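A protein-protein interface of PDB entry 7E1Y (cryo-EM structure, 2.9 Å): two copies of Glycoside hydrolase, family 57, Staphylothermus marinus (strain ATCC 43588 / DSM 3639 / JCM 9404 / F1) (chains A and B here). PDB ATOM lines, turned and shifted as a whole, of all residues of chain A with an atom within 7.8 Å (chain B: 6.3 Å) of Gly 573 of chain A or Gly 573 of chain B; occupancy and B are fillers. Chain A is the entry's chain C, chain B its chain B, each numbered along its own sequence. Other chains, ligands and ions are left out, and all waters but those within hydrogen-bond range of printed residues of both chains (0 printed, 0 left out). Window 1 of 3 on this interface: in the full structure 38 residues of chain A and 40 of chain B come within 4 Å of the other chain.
OG of Ser 613 of chain A sits close to OG1 of Thr 574 of chain B. The backbone carbonyl oxygen (O) of Ala 570 of chain A is in hydrogen-bond range of the side-chain hydroxyl (OG1) of Thr 574 of chain B (3.1 Å). The backbone carbonyl oxygen (O) of Ile 571 of chain A sits close to the backbone carbonyl oxygen (O) of Thr 574 of chain B.
Ile 571 of chain A touches Thr 574 of chain B, and with the chains exchanged Thr 574 of chain A touches Ile 571 of chain B. Gly 572 of chain A touches Gly 573 of chain B, and with the chains exchanged Gly 573 of chain A touches Gly 572 of chain B. Gly 572 of chain A touches Thr 574 of chain B, and with the chains exchanged Thr 574 of chain A touches Gly 572 of chain B. Val 611 of chain B touches its own counterpart, Val 611 of chain A. Positions printed for both chains: 571, 572, 573, 574, 575, 576, 609, 610 and 611.
Gly 573 of chain A touches two residues of chain B. Printed residues of chain B within 4 Å of Thr 574 of chain A: Ile 571 and Gly 572. Phe 576 of chain A touches none of the printed residues of chain B. Of the printed residues of chain B, Val 611 of chain A touches Lys 609 and Val 611. Of the printed residues of chain B, Ile 620 of chain A touches Thr 574 (3.7 Å). Of the printed residues of chain A, Ile 571 of chain B touches Thr 574. Of chain A, only Gly 573 and Thr 574 come within 4 Å of Gly 572 of chain B. Gly 573 of chain B touches two residues of chain A. Phe 576 of chain B touches none of the printed residues of chain A.
Hydrophobic or aromatic side chains of chain A within 4 Å of the printed part of chain B: Ala 570, Val 611 and Ile 620. Of the 9 printed residues of chain B, 6 touch a printed residue of chain A. Hydrophobic or aromatic side chains of chain B within 4 Å of the printed part of chain A: Val 611. Along chain B the printed residues that touch a printed residue of chain A span positions 571 to 611.
Gly 572 of chain A touches Gly 573 of chain B. Thr 574 of chain B touches Gly 572 of chain A. Gly 573 of chain A touches Gly 572 of chain B. Gly 573 of chain B touches Gly 573 of chain A (N to N, 3.8 Å). CA of Thr 574 of chain A touches O of Ile 571 of chain B, at 3.6 Å. CA of Gly 572 of chain B touches N of Thr 574 of chain A (3.8 Å). Lys 609 of chain A touches Val 611 of chain B. Lys 609 of chain B touches Val 611 of chain A (CB to CG1, 3.9 Å). Val 611 of chain B touches Val 611 of chain A (CG2 to CG2, 3.6 Å). Ile 620 of chain A touches Thr 574 of chain B.
The backbone carbonyl oxygen (O) of Gly 572 of chain B lies within hydrogen-bond range of the backbone NH (N) of Val 611 of chain B, 2.5 Å away. N of Ala 570 of chain A lies within hydrogen-bond range of O of Ser 613 of chain A, 2.7 Å away. O of Val 611 of chain A lies within hydrogen-bond range of N of Gly 572 of chain A.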
ATOM      1  N   ALA A 570      16.585   6.492 -18.428  1.00  0.00           N
ATOM      2  CA  ALA A 570      16.689   5.586 -17.296  1.00  0.00           C
ATOM      3  C   ALA A 570      16.033   6.226 -16.085  1.00  0.00           C
ATOM      4  O   ALA A 570      16.092   7.445 -15.906  1.00  0.00           O
ATOM      5  CB  ALA A 570      18.145   5.240 -16.978  1.00  0.00           C
ATOM      6  N   ILE A 571      15.409   5.395 -15.254  1.00  0.00           N
ATOM      7  CA  ILE A 571      14.721   5.876 -14.063  1.00  0.00           C
ATOM      8  C   ILE A 571      15.665   5.784 -12.874  1.00  0.00           C
ATOM      9  O   ILE A 571      16.703   5.117 -12.937  1.00  0.00           O
ATOM     10  CB  ILE A 571      13.429   5.082 -13.801  1.00  0.00           C
ATOM     11  CG1 ILE A 571      13.764   3.642 -13.408  1.00  0.00           C
ATOM     12  CG2 ILE A 571      12.529   5.111 -15.026  1.00  0.00           C
ATOM     13  CD1 ILE A 571      12.729   2.998 -12.517  1.00  0.00           C
ATOM     14  N   GLY A 572      15.310   6.453 -11.786  1.00  0.00           N
ATOM     15  CA  GLY A 572      16.119   6.410 -10.584  1.00  0.00           C
ATOM     16  C   GLY A 572      15.268   6.763  -9.389  1.00  0.00           C
ATOM     17  O   GLY A 572      14.202   7.374  -9.510  1.00  0.00           O
ATOM     18  N   GLY A 573      15.759   6.371  -8.227  1.00  0.00           N
ATOM     19  CA  GLY A 573      15.026   6.579  -6.999  1.00  0.00           C
ATOM     20  C   GLY A 573      15.517   5.639  -5.923  1.00  0.00           C
ATOM     21  O   GLY A 573      16.129   4.605  -6.192  1.00  0.00           O
ATOM     22  N   THR A 574      15.224   6.027  -4.684  1.00  0.00           N
ATOM     23  CA  THR A 574      15.762   5.314  -3.532  1.00  0.00           C
ATOM     24  C   THR A 574      15.229   3.888  -3.441  1.00  0.00           C
ATOM     25  O   THR A 574      15.986   2.959  -3.138  1.00  0.00           O
ATOM     26  CB  THR A 574      15.459   6.098  -2.259  1.00  0.00           C
ATOM     27  OG1 THR A 574      15.913   5.364  -1.116  1.00  0.00           O
ATOM     28  CG2 THR A 574      13.966   6.396  -2.134  1.00  0.00           C
ATOM     29  N   GLY A 575      13.939   3.691  -3.697  1.00  0.00           N
ATOM     30  CA  GLY A 575      13.368   2.363  -3.622  1.00  0.00           C
ATOM     31  C   GLY A 575      12.820   1.878  -4.944  1.00  0.00           C
ATOM     32  O   GLY A 575      12.637   0.674  -5.147  1.00  0.00           O
ATOM     33  N   PHE A 576      12.557   2.811  -5.855  1.00  0.00           N
ATOM     34  CA  PHE A 576      11.968   2.466  -7.140  1.00  0.00           C
ATOM     35  C   PHE A 576      12.921   1.621  -7.966  1.00  0.00           C
ATOM     36  O   PHE A 576      14.114   1.917  -8.067  1.00  0.00           O
ATOM     37  CB  PHE A 576      11.597   3.735  -7.903  1.00  0.00           C
ATOM     38  CG  PHE A 576      10.444   4.470  -7.308  1.00  0.00           C
ATOM     39  CD1 PHE A 576       9.206   3.865  -7.203  1.00  0.00           C
ATOM     40  CD2 PHE A 576      10.592   5.764  -6.855  1.00  0.00           C
ATOM     41  CE1 PHE A 576       8.141   4.536  -6.654  1.00  0.00           C
ATOM     42  CE2 PHE A 576       9.528   6.440  -6.311  1.00  0.00           C
ATOM     43  CZ  PHE A 576       8.301   5.825  -6.209  1.00  0.00           C
ATOM     44  N   SER A 577      12.381   0.563  -8.563  1.00  0.00           N
ATOM     45  CA  SER A 577      13.160  -0.357  -9.383  1.00  0.00           C
ATOM     46  C   SER A 577      12.313  -0.742 -10.586  1.00  0.00           C
ATOM     47  O   SER A 577      11.279  -1.399 -10.430  1.00  0.00           O
ATOM     48  CB  SER A 577      13.574  -1.594  -8.586  1.00  0.00           C
ATOM     49  OG  SER A 577      12.441  -2.359  -8.214  1.00  0.00           O
ATOM     50  N   PHE A 604       9.771   0.800  -0.165  1.00  0.00           N
ATOM     51  CA  PHE A 604       9.396   1.419   1.092  1.00  0.00           C
ATOM     52  C   PHE A 604       8.077   2.164   0.918  1.00  0.00           C
ATOM     53  O   PHE A 604       7.539   2.276  -0.184  1.00  0.00           O
ATOM     54  CB  PHE A 604      10.503   2.356   1.570  1.00  0.00           C
ATOM     55  CG  PHE A 604      11.873   1.754   1.496  1.00  0.00           C
ATOM     56  CD1 PHE A 604      12.239   0.723   2.341  1.00  0.00           C
ATOM     57  CD2 PHE A 604      12.792   2.212   0.569  1.00  0.00           C
ATOM     58  CE1 PHE A 604      13.497   0.169   2.268  1.00  0.00           C
ATOM     59  CE2 PHE A 604      14.049   1.659   0.491  1.00  0.00           C
ATOM     60  CZ  PHE A 604      14.401   0.636   1.341  1.00  0.00           C
ATOM     61  N   HIS A 608       8.453   9.582  -1.519  1.00  0.00           N
ATOM     62  CA  HIS A 608       9.506   9.124  -2.413  1.00  0.00           C
ATOM     63  C   HIS A 608       9.941  10.225  -3.373  1.00  0.00           C
ATOM     64  O   HIS A 608       9.149  11.069  -3.793  1.00  0.00           O
ATOM     65  CB  HIS A 608       9.046   7.920  -3.233  1.00  0.00           C
ATOM     66  CG  HIS A 608       9.054   6.627  -2.485  1.00  0.00           C
ATOM     67  ND1 HIS A 608       9.698   5.504  -2.955  1.00  0.00           N
ATOM     68  CD2 HIS A 608       8.473   6.265  -1.318  1.00  0.00           C
ATOM     69  CE1 HIS A 608       9.525   4.511  -2.103  1.00  0.00           C
ATOM     70  NE2 HIS A 608       8.783   4.946  -1.102  1.00  0.00           N
ATOM     71  N   LYS A 609      11.220  10.188  -3.733  1.00  0.00           N
ATOM     72  CA  LYS A 609      11.791  11.038  -4.775  1.00  0.00           C
ATOM     73  C   LYS A 609      12.210  10.126  -5.921  1.00  0.00           C
ATOM     74  O   LYS A 609      12.979   9.182  -5.718  1.00  0.00           O
ATOM     75  CB  LYS A 609      12.971  11.846  -4.248  1.00  0.00           C
ATOM     76  CG  LYS A 609      12.627  12.795  -3.124  1.00  0.00           C
ATOM     77  CD  LYS A 609      11.760  13.933  -3.622  1.00  0.00           C
ATOM     78  CE  LYS A 609      11.411  14.878  -2.493  1.00  0.00           C
ATOM     79  NZ  LYS A 609      12.608  15.612  -2.003  1.00  0.00           N
ATOM     80  N   MET A 610      11.704  10.396  -7.117  1.00  0.00           N
ATOM     81  CA  MET A 610      12.029   9.576  -8.275  1.00  0.00           C
ATOM     82  C   MET A 610      12.654  10.422  -9.376  1.00  0.00           C
ATOM     83  O   MET A 610      12.149  11.494  -9.719  1.00  0.00           O
ATOM     84  CB  MET A 610      10.776   8.876  -8.793  1.00  0.00           C
ATOM     85  CG  MET A 610      11.034   7.919  -9.932  1.00  0.00           C
ATOM     86  SD  MET A 610       9.680   6.761 -10.166  1.00  0.00           S
ATOM     87  CE  MET A 610      10.522   5.431 -11.012  1.00  0.00           C
ATOM     88  N   VAL A 611      13.759   9.930  -9.931  1.00  0.00           N
ATOM     89  CA  VAL A 611      14.527  10.640 -10.946  1.00  0.00           C
ATOM     90  C   VAL A 611      14.387   9.907 -12.271  1.00  0.00           C
ATOM     91  O   VAL A 611      14.577   8.687 -12.333  1.00  0.00           O
ATOM     92  CB  VAL A 611      16.010  10.763 -10.556  1.00  0.00           C
ATOM     93  CG1 VAL A 611      16.775  11.513 -11.632  1.00  0.00           C
ATOM     94  CG2 VAL A 611      16.149  11.458  -9.221  1.00  0.00           C
ATOM     95  N   VAL A 612      14.054  10.648 -13.322  1.00  0.00           N
ATOM     96  CA  VAL A 612      14.029  10.136 -14.685  1.00  0.00           C
ATOM     97  C   VAL A 612      14.990  10.972 -15.513  1.00  0.00           C
ATOM     98  O   VAL A 612      14.887  12.203 -15.532  1.00  0.00           O
ATOM     99  CB  VAL A 612      12.611  10.175 -15.285  1.00  0.00           C
ATOM    100  CG1 VAL A 612      12.595   9.506 -16.651  1.00  0.00           C
ATOM    101  CG2 VAL A 612      11.617   9.508 -14.346  1.00  0.00           C
ATOM    102  N   SER A 613      15.920  10.309 -16.192  1.00  0.00           N
ATOM    103  CA  SER A 613      16.962  10.998 -16.936  1.00  0.00           C
ATOM    104  C   SER A 613      17.083  10.404 -18.328  1.00  0.00           C
ATOM    105  O   SER A 613      17.087   9.182 -18.488  1.00  0.00           O
ATOM    106  CB  SER A 613      18.309  10.901 -16.224  1.00  0.00           C
ATOM    107  OG  SER A 613      18.754   9.562 -16.201  1.00  0.00           O
ATOM    108  N   ILE A 620      24.066  11.576 -20.097  1.00  0.00           N
ATOM    109  CA  ILE A 620      22.782  12.057 -19.606  1.00  0.00           C
ATOM    110  C   ILE A 620      22.481  13.403 -20.247  1.00  0.00           C
ATOM    111  O   ILE A 620      23.195  14.388 -20.026  1.00  0.00           O
ATOM    112  CB  ILE A 620      22.779  12.156 -18.077  1.00  0.00           C
ATOM    113  CG1 ILE A 620      22.655  10.768 -17.460  1.00  0.00           C
ATOM    114  CG2 ILE A 620      21.639  13.032 -17.601  1.00  0.00           C
ATOM    115  CD1 ILE A 620      22.836  10.760 -15.979  1.00  0.00           C
ATOM    116  N   ILE B 571      20.312   5.039  -0.813  1.00  0.00           N
ATOM    117  CA  ILE B 571      20.556   6.080  -1.805  1.00  0.00           C
ATOM    118  C   ILE B 571      19.775   5.769  -3.073  1.00  0.00           C
ATOM    119  O   ILE B 571      19.297   4.645  -3.267  1.00  0.00           O
ATOM    120  CB  ILE B 571      22.057   6.226  -2.110  1.00  0.00           C
ATOM    121  CG1 ILE B 571      22.556   5.015  -2.901  1.00  0.00           C
ATOM    122  CG2 ILE B 571      22.849   6.395  -0.823  1.00  0.00           C
ATOM    123  CD1 ILE B 571      23.707   5.330  -3.824  1.00  0.00           C
ATOM    124  N   GLY B 572      19.640   6.762  -3.939  1.00  0.00           N
ATOM    125  CA  GLY B 572      18.970   6.563  -5.207  1.00  0.00           C
ATOM    126  C   GLY B 572      19.589   7.456  -6.259  1.00  0.00           C
ATOM    127  O   GLY B 572      20.170   8.503  -5.959  1.00  0.00           O
ATOM    128  N   GLY B 573      19.453   7.020  -7.500  1.00  0.00           N
ATOM    129  CA  GLY B 573      20.019   7.752  -8.610  1.00  0.00           C
ATOM    130  C   GLY B 573      19.711   7.049  -9.916  1.00  0.00           C
ATOM    131  O   GLY B 573      19.346   5.875  -9.943  1.00  0.00           O
ATOM    132  N   THR B 574      19.870   7.805 -11.000  1.00  0.00           N
ATOM    133  CA  THR B 574      19.478   7.299 -12.310  1.00  0.00           C
ATOM    134  C   THR B 574      20.467   6.261 -12.831  1.00  0.00           C
ATOM    135  O   THR B 574      20.089   5.375 -13.604  1.00  0.00           O
ATOM    136  CB  THR B 574      19.329   8.460 -13.291  1.00  0.00           C
ATOM    137  OG1 THR B 574      18.836   7.973 -14.545  1.00  0.00           O
ATOM    138  CG2 THR B 574      20.662   9.167 -13.500  1.00  0.00           C
ATOM    139  N   GLY B 575      21.731   6.348 -12.422  1.00  0.00           N
ATOM    140  CA  GLY B 575      22.722   5.388 -12.866  1.00  0.00           C
ATOM    141  C   GLY B 575      23.616   4.872 -11.758  1.00  0.00           C
ATOM    142  O   GLY B 575      24.480   4.023 -11.992  1.00  0.00           O
ATOM    143  N   PHE B 576      23.413   5.376 -10.545  1.00  0.00           N
ATOM    144  CA  PHE B 576      24.297   5.052  -9.433  1.00  0.00           C
ATOM    145  C   PHE B 576      24.030   3.654  -8.893  1.00  0.00           C
ATOM    146  O   PHE B 576      22.928   3.117  -9.037  1.00  0.00           O
ATOM    147  CB  PHE B 576      24.126   6.087  -8.329  1.00  0.00           C
ATOM    148  CG  PHE B 576      24.665   7.435  -8.686  1.00  0.00           C
ATOM    149  CD1 PHE B 576      26.019   7.614  -8.901  1.00  0.00           C
ATOM    150  CD2 PHE B 576      23.818   8.517  -8.832  1.00  0.00           C
ATOM    151  CE1 PHE B 576      26.523   8.849  -9.228  1.00  0.00           C
ATOM    152  CE2 PHE B 576      24.316   9.756  -9.161  1.00  0.00           C
ATOM    153  CZ  PHE B 576      25.671   9.923  -9.358  1.00  0.00           C
ATOM    154  N   LYS B 609      21.753  13.001 -10.829  1.00  0.00           N
ATOM    155  CA  LYS B 609      20.947  13.421  -9.682  1.00  0.00           C
ATOM    156  C   LYS B 609      20.949  12.285  -8.665  1.00  0.00           C
ATOM    157  O   LYS B 609      20.417  11.204  -8.932  1.00  0.00           O
ATOM    158  CB  LYS B 609      19.528  13.781 -10.107  1.00  0.00           C
ATOM    159  CG  LYS B 609      19.450  14.766 -11.253  1.00  0.00           C
ATOM    160  CD  LYS B 609      20.108  16.083 -10.903  1.00  0.00           C
ATOM    161  CE  LYS B 609      19.241  16.904  -9.975  1.00  0.00           C
ATOM    162  NZ  LYS B 609      18.016  17.377 -10.667  1.00  0.00           N
ATOM    163  N   MET B 610      21.547  12.532  -7.503  1.00  0.00           N
ATOM    164  CA  MET B 610      21.567  11.568  -6.412  1.00  0.00           C
ATOM    165  C   MET B 610      20.452  11.862  -5.419  1.00  0.00           C
ATOM    166  O   MET B 610      20.298  12.995  -4.960  1.00  0.00           O
ATOM    167  CB  MET B 610      22.908  11.603  -5.676  1.00  0.00           C
ATOM    168  CG  MET B 610      23.047  10.537  -4.596  1.00  0.00           C
ATOM    169  SD  MET B 610      23.514   8.884  -5.125  1.00  0.00           S
ATOM    170  CE  MET B 610      25.135   9.209  -5.807  1.00  0.00           C
ATOM    171  N   VAL B 611      19.684  10.832  -5.084  1.00  0.00           N
ATOM    172  CA  VAL B 611      18.692  10.900  -4.019  1.00  0.00           C
ATOM    173  C   VAL B 611      19.176  10.034  -2.870  1.00  0.00           C
ATOM    174  O   VAL B 611      19.500   8.859  -3.068  1.00  0.00           O
ATOM    175  CB  VAL B 611      17.302  10.439  -4.494  1.00  0.00           C
ATOM    176  CG1 VAL B 611      16.308  10.530  -3.354  1.00  0.00           C
ATOM    177  CG2 VAL B 611      16.839  11.268  -5.671  1.00  0.00           C
